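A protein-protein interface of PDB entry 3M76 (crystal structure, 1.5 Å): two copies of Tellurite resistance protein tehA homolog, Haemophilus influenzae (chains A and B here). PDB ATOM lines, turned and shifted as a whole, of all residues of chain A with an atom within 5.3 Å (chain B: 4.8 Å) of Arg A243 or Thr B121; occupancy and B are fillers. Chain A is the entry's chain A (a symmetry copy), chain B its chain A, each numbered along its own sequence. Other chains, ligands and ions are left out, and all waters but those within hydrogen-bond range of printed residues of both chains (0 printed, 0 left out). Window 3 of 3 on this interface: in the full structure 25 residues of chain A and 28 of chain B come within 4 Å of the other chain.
Of the 9 printed residues of chain B, 5 touch a printed residue of chain A.
Along chain B the printed residues that touch a printed residue of chain A span positions 120 to 126.
Among the printed residues, Asp or Glu carboxylates within 4 Å of a Lys or Arg side-chain nitrogen of the other chain: Arg A243 with Glu B126 (3.7 Å).
Among the printed residues, pairs that only touch across the chains: Phe A239 with Thr B121 (3.7 Å), Phe A240 with Ser B120 (3.6 Å), Phe A240 with Thr B121 (3.8 Å), Phe A240 with Ser B125 (3.6 Å), Arg A243 with Thr B121 (3.3 Å), Arg A243 with Ser B125 (3.2 Å) and Leu A244 with Ser B125 (3.5 Å).
The side-chain hydroxyl (OG) of Ser B120 lies within hydrogen-bond range of the backbone carbonyl oxygen (O) of Leu B117, at 3.2 Å.
O of Leu B117 lies within hydrogen-bond range of OG1 of Thr B121 (2.8 Å).
O of Ser B120 lies within hydrogen-bond range of N of Ser B125 (3.4 Å).
OG of Ser B125 is in hydrogen-bond range of O of Thr B121 (2.6 Å).
The side-chain carboxylate (OE1) of Glu B126 lies within salt-bridge range of the guanidinium group (NH1) of Arg B123 (2.8 Å).
Of the printed residues of chain B, Arg A243 touches Thr B121 (3.3 Å), Leu B122 (2.8 Å), Ser B125 (3.2 Å) and Glu B126 (3.7 Å).
Printed residues of chain A within 4 Å of Ser B120: Phe A240.
Printed residues of chain A within 4 Å of Leu B122: Arg A243 (2.8 Å).
Of the printed residues of chain A, Glu B126 touches Arg A243.
Phe B119 touches none of the printed residues of chain A.
Leu B117 touches none of the printed residues of chain A.
The nearest printed residue of chain B that does not touch Phe A240 is Leu B117 (5.7 Å).
No position is printed for both chains.
Of the 9 pairs that touch across the chains among the printed residues, none has its exchanged pair printed and touching as well.
The guanidinium group of Arg A243 sits at hydrogen-bond distance from the backbone carbonyl oxygen of Leu B122, at 2.8 Å.
NH2 of Arg A243 is in salt-bridge range of OE1 of Glu B126.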
ATOM      1  N   LEU A 238      12.851  -6.705 -34.001  1.00  0.00           N
ATOM      2  CA  LEU A 238      11.865  -7.385 -34.886  1.00  0.00           C
ATOM      3  C   LEU A 238      11.329  -8.653 -34.210  1.00  0.00           C
ATOM      4  O   LEU A 238      10.126  -8.891 -34.181  1.00  0.00           O
ATOM      5  CB  LEU A 238      12.513  -7.759 -36.224  1.00  0.00           C
ATOM      6  CG  LEU A 238      11.625  -8.601 -37.146  1.00  0.00           C
ATOM      7  CD1 LEU A 238      10.410  -7.814 -37.556  1.00  0.00           C
ATOM      8  CD2 LEU A 238      12.444  -9.062 -38.353  1.00  0.00           C
ATOM      9  N   PHE A 239      12.216  -9.482 -33.678  1.00  0.00           N
ATOM     10  CA  PHE A 239      11.793 -10.716 -33.036  1.00  0.00           C
ATOM     11  C   PHE A 239      10.890 -10.416 -31.847  1.00  0.00           C
ATOM     12  O   PHE A 239       9.878 -11.080 -31.625  1.00  0.00           O
ATOM     13  CB  PHE A 239      12.992 -11.556 -32.591  1.00  0.00           C
ATOM     14  CG  PHE A 239      13.866 -12.063 -33.712  1.00  0.00           C
ATOM     15  CD1 PHE A 239      13.451 -12.072 -35.003  1.00  0.00           C
ATOM     16  CD2 PHE A 239      15.171 -12.315 -33.460  1.00  0.00           C
ATOM     17  CE1 PHE A 239      14.280 -12.509 -36.016  1.00  0.00           C
ATOM     18  CE2 PHE A 239      16.015 -12.734 -34.464  1.00  0.00           C
ATOM     19  CZ  PHE A 239      15.556 -12.841 -35.726  1.00  0.00           C
ATOM     20  N   PHE A 240      11.263  -9.404 -31.061  1.00  0.00           N
ATOM     21  CA  PHE A 240      10.456  -9.026 -29.904  1.00  0.00           C
ATOM     22  C   PHE A 240       9.047  -8.603 -30.355  1.00  0.00           C
ATOM     23  O   PHE A 240       8.036  -8.990 -29.765  1.00  0.00           O
ATOM     24  CB  PHE A 240      11.109  -7.865 -29.133  1.00  0.00           C
ATOM     25  CG  PHE A 240      12.298  -8.252 -28.289  1.00  0.00           C
ATOM     26  CD1 PHE A 240      12.824  -9.525 -28.296  1.00  0.00           C
ATOM     27  CD2 PHE A 240      12.903  -7.320 -27.482  1.00  0.00           C
ATOM     28  CE1 PHE A 240      13.914  -9.858 -27.485  1.00  0.00           C
ATOM     29  CE2 PHE A 240      13.985  -7.674 -26.702  1.00  0.00           C
ATOM     30  CZ  PHE A 240      14.475  -8.914 -26.711  1.00  0.00           C
ATOM     31  N   LEU A 241       8.979  -7.782 -31.405  1.00  0.00           N
ATOM     32  CA  LEU A 241       7.705  -7.259 -31.889  1.00  0.00           C
ATOM     33  C   LEU A 241       6.863  -8.357 -32.523  1.00  0.00           C
ATOM     34  O   LEU A 241       5.635  -8.338 -32.410  1.00  0.00           O
ATOM     35  CB  LEU A 241       7.922  -6.089 -32.846  1.00  0.00           C
ATOM     36  CG  LEU A 241       8.419  -4.833 -32.133  1.00  0.00           C
ATOM     37  CD1 LEU A 241       8.979  -3.863 -33.139  1.00  0.00           C
ATOM     38  CD2 LEU A 241       7.323  -4.159 -31.304  1.00  0.00           C
ATOM     39  N   LEU A 242       7.506  -9.323 -33.186  1.00  0.00           N
ATOM     40  CA  LEU A 242       6.778 -10.479 -33.703  1.00  0.00           C
ATOM     41  C   LEU A 242       6.123 -11.247 -32.563  1.00  0.00           C
ATOM     42  O   LEU A 242       4.941 -11.640 -32.646  1.00  0.00           O
ATOM     43  CB  LEU A 242       7.725 -11.389 -34.487  1.00  0.00           C
ATOM     44  CG  LEU A 242       8.077 -10.876 -35.884  1.00  0.00           C
ATOM     45  CD1 LEU A 242       9.195 -11.708 -36.402  1.00  0.00           C
ATOM     46  CD2 LEU A 242       6.874 -11.027 -36.804  1.00  0.00           C
ATOM     47  N   ARG A 243       6.865 -11.476 -31.487  1.00  0.00           N
ATOM     48  CA  ARG A 243       6.321 -12.178 -30.331  1.00  0.00           C
ATOM     49  C   ARG A 243       5.148 -11.403 -29.729  1.00  0.00           C
ATOM     50  O   ARG A 243       4.129 -11.992 -29.314  1.00  0.00           O
ATOM     51  CB  ARG A 243       7.420 -12.460 -29.314  1.00  0.00           C
ATOM     52  CG  ARG A 243       7.021 -13.316 -28.144  1.00  0.00           C
ATOM     53  CD  ARG A 243       6.411 -12.524 -26.989  1.00  0.00           C
ATOM     54  NE  ARG A 243       6.388 -13.297 -25.744  1.00  0.00           N
ATOM     55  CZ  ARG A 243       5.396 -14.038 -25.350  1.00  0.00           C
ATOM     56  NH1 ARG A 243       4.291 -14.088 -26.096  1.00  0.00           N
ATOM     57  NH2 ARG A 243       5.494 -14.708 -24.216  1.00  0.00           N
ATOM     58  N   LEU A 244       5.284 -10.098 -29.706  1.00  0.00           N
ATOM     59  CA  LEU A 244       4.284  -9.205 -29.156  1.00  0.00           C
ATOM     60  C   LEU A 244       3.101  -8.953 -30.061  1.00  0.00           C
ATOM     61  O   LEU A 244       2.117  -8.324 -29.630  1.00  0.00           O
ATOM     62  CB  LEU A 244       4.920  -7.867 -28.810  1.00  0.00           C
ATOM     63  CG  LEU A 244       5.827  -7.901 -27.577  1.00  0.00           C
ATOM     64  CD1 LEU A 244       6.619  -6.625 -27.517  1.00  0.00           C
ATOM     65  CD2 LEU A 244       5.004  -8.085 -26.313  1.00  0.00           C
ATOM     66  N   PHE A 245       3.147  -9.421 -31.300  1.00  0.00           N
ATOM     67  CA  PHE A 245       2.126  -9.019 -32.263  1.00  0.00           C
ATOM     68  C   PHE A 245       0.682  -9.351 -31.853  1.00  0.00           C
ATOM     69  O   PHE A 245      -0.188  -8.492 -31.979  1.00  0.00           O
ATOM     70  CB  PHE A 245       2.457  -9.504 -33.677  1.00  0.00           C
ATOM     71  CG  PHE A 245       1.650  -8.809 -34.740  1.00  0.00           C
ATOM     72  CD1 PHE A 245       2.046  -7.569 -35.186  1.00  0.00           C
ATOM     73  CD2 PHE A 245       0.497  -9.381 -35.258  1.00  0.00           C
ATOM     74  CE1 PHE A 245       1.337  -6.909 -36.140  1.00  0.00           C
ATOM     75  CE2 PHE A 245      -0.227  -8.699 -36.237  1.00  0.00           C
ATOM     76  CZ  PHE A 245       0.209  -7.474 -36.661  1.00  0.00           C
ATOM     77  N   PRO A 246       0.444 -10.555 -31.324  1.00  0.00           N
ATOM     78  CA  PRO A 246      -0.948 -10.858 -30.888  1.00  0.00           C
ATOM     79  C   PRO A 246      -1.471  -9.869 -29.859  1.00  0.00           C
ATOM     80  O   PRO A 246      -2.652  -9.477 -29.911  1.00  0.00           O
ATOM     81  CB  PRO A 246      -0.829 -12.266 -30.298  1.00  0.00           C
ATOM     82  CG  PRO A 246       0.268 -12.887 -31.044  1.00  0.00           C
ATOM     83  CD  PRO A 246       1.315 -11.751 -31.229  1.00  0.00           C
ATOM     84  N   LEU B 117      18.344 -16.907 -27.414  1.00  0.00           N
ATOM     85  CA  LEU B 117      17.578 -16.036 -28.277  1.00  0.00           C
ATOM     86  C   LEU B 117      16.083 -16.328 -28.102  1.00  0.00           C
ATOM     87  O   LEU B 117      15.259 -15.401 -28.018  1.00  0.00           O
ATOM     88  CB  LEU B 117      18.032 -16.157 -29.728  1.00  0.00           C
ATOM     89  CG  LEU B 117      17.345 -15.252 -30.733  1.00  0.00           C
ATOM     90  CD1 LEU B 117      17.474 -13.762 -30.369  1.00  0.00           C
ATOM     91  CD2 LEU B 117      17.845 -15.575 -32.144  1.00  0.00           C
ATOM     92  N   LEU B 118      15.708 -17.616 -28.051  1.00  0.00           N
ATOM     93  CA  LEU B 118      14.308 -17.978 -27.807  1.00  0.00           C
ATOM     94  C   LEU B 118      13.848 -17.446 -26.440  1.00  0.00           C
ATOM     95  O   LEU B 118      12.769 -16.880 -26.304  1.00  0.00           O
ATOM     96  CB  LEU B 118      14.125 -19.471 -27.859  1.00  0.00           C
ATOM     97  CG  LEU B 118      12.782 -20.020 -27.512  1.00  0.00           C
ATOM     98  CD1 LEU B 118      11.767 -19.491 -28.545  1.00  0.00           C
ATOM     99  CD2 LEU B 118      12.839 -21.544 -27.518  1.00  0.00           C
ATOM    100  N   PHE B 119      14.693 -17.627 -25.433  1.00  0.00           N
ATOM    101  CA  PHE B 119      14.410 -17.152 -24.073  1.00  0.00           C
ATOM    102  C   PHE B 119      14.109 -15.674 -24.020  1.00  0.00           C
ATOM    103  O   PHE B 119      13.096 -15.246 -23.471  1.00  0.00           O
ATOM    104  CB  PHE B 119      15.564 -17.523 -23.134  1.00  0.00           C
ATOM    105  CG  PHE B 119      15.309 -17.174 -21.696  1.00  0.00           C
ATOM    106  CD1 PHE B 119      14.439 -17.909 -20.950  1.00  0.00           C
ATOM    107  CD2 PHE B 119      15.938 -16.125 -21.090  1.00  0.00           C
ATOM    108  CE1 PHE B 119      14.214 -17.593 -19.637  1.00  0.00           C
ATOM    109  CE2 PHE B 119      15.686 -15.810 -19.771  1.00  0.00           C
ATOM    110  CZ  PHE B 119      14.820 -16.555 -19.050  1.00  0.00           C
ATOM    111  N   SER B 120      14.991 -14.860 -24.592  1.00  0.00           N
ATOM    112  CA  SER B 120      14.792 -13.415 -24.556  1.00  0.00           C
ATOM    113  C   SER B 120      13.586 -13.028 -25.391  1.00  0.00           C
ATOM    114  O   SER B 120      12.773 -12.199 -24.970  1.00  0.00           O
ATOM    115  CB  SER B 120      16.032 -12.664 -25.043  1.00  0.00           C
ATOM    116  OG  SER B 120      16.264 -12.873 -26.428  1.00  0.00           O
ATOM    117  N   THR B 121      13.458 -13.617 -26.578  1.00  0.00           N
ATOM    118  CA  THR B 121      12.332 -13.315 -27.442  1.00  0.00           C
ATOM    119  C   THR B 121      11.017 -13.610 -26.755  1.00  0.00           C
ATOM    120  O   THR B 121      10.034 -12.865 -26.931  1.00  0.00           O
ATOM    121  CB  THR B 121      12.439 -14.095 -28.775  1.00  0.00           C
ATOM    122  OG1 THR B 121      13.602 -13.618 -29.472  1.00  0.00           O
ATOM    123  CG2 THR B 121      11.211 -13.871 -29.626  1.00  0.00           C
ATOM    124  N   LEU B 122      10.967 -14.676 -25.973  1.00  0.00           N
ATOM    125  CA  LEU B 122       9.734 -14.979 -25.255  1.00  0.00           C
ATOM    126  C   LEU B 122       9.523 -14.095 -24.018  1.00  0.00           C
ATOM    127  O   LEU B 122       8.423 -13.558 -23.808  1.00  0.00           O
ATOM    128  CB  LEU B 122       9.738 -16.422 -24.814  1.00  0.00           C
ATOM    129  CG  LEU B 122       9.556 -17.419 -25.954  1.00  0.00           C
ATOM    130  CD1 LEU B 122       9.822 -18.843 -25.475  1.00  0.00           C
ATOM    131  CD2 LEU B 122       8.181 -17.293 -26.541  1.00  0.00           C
ATOM    132  N   ARG B 123      10.564 -13.912 -23.215  1.00  0.00           N
ATOM    133  CA  ARG B 123      10.394 -13.269 -21.911  1.00  0.00           C
ATOM    134  C   ARG B 123      10.736 -11.816 -21.826  1.00  0.00           C
ATOM    135  O   ARG B 123      10.045 -11.067 -21.138  1.00  0.00           O
ATOM    136  CB  ARG B 123      11.172 -14.013 -20.834  1.00  0.00           C
ATOM    137  CG  ARG B 123      10.487 -15.252 -20.499  1.00  0.00           C
ATOM    138  CD  ARG B 123       9.132 -14.991 -19.829  1.00  0.00           C
ATOM    139  NE  ARG B 123       9.356 -14.385 -18.523  1.00  0.00           N
ATOM    140  CZ  ARG B 123       8.861 -13.233 -18.099  1.00  0.00           C
ATOM    141  NH1 ARG B 123       7.987 -12.547 -18.817  1.00  0.00           N
ATOM    142  NH2 ARG B 123       9.197 -12.800 -16.906  1.00  0.00           N
ATOM    143  N   SER B 125      10.755  -9.533 -24.235  1.00  0.00           N
ATOM    144  CA  SER B 125       9.726  -8.799 -24.954  1.00  0.00           C
ATOM    145  C   SER B 125       8.410  -8.752 -24.193  1.00  0.00           C
ATOM    146  O   SER B 125       7.734  -7.729 -24.219  1.00  0.00           O
ATOM    147  CB  SER B 125       9.488  -9.424 -26.320  1.00  0.00           C
ATOM    148  OG  SER B 125       8.844 -10.655 -26.184  1.00  0.00           O
ATOM    149  N   GLU B 126       8.056  -9.841 -23.498  1.00  0.00           N
ATOM    150  CA  GLU B 126       6.799  -9.895 -22.806  1.00  0.00           C
ATOM    151  C   GLU B 126       6.688  -8.792 -21.754  1.00  0.00           C
ATOM    152  O   GLU B 126       5.595  -8.315 -21.442  1.00  0.00           O
ATOM    153  CB  GLU B 126       6.656 -11.266 -22.136  1.00  0.00           C
ATOM    154  CG  GLU B 126       5.317 -11.505 -21.544  1.00  0.00           C
ATOM    155  CD  GLU B 126       5.146 -12.929 -20.989  1.00  0.00           C
ATOM    156  OE1 GLU B 126       6.154 -13.623 -20.695  1.00  0.00           O
ATOM    157  OE2 GLU B 126       3.957 -13.343 -20.819  1.00  0.00           O
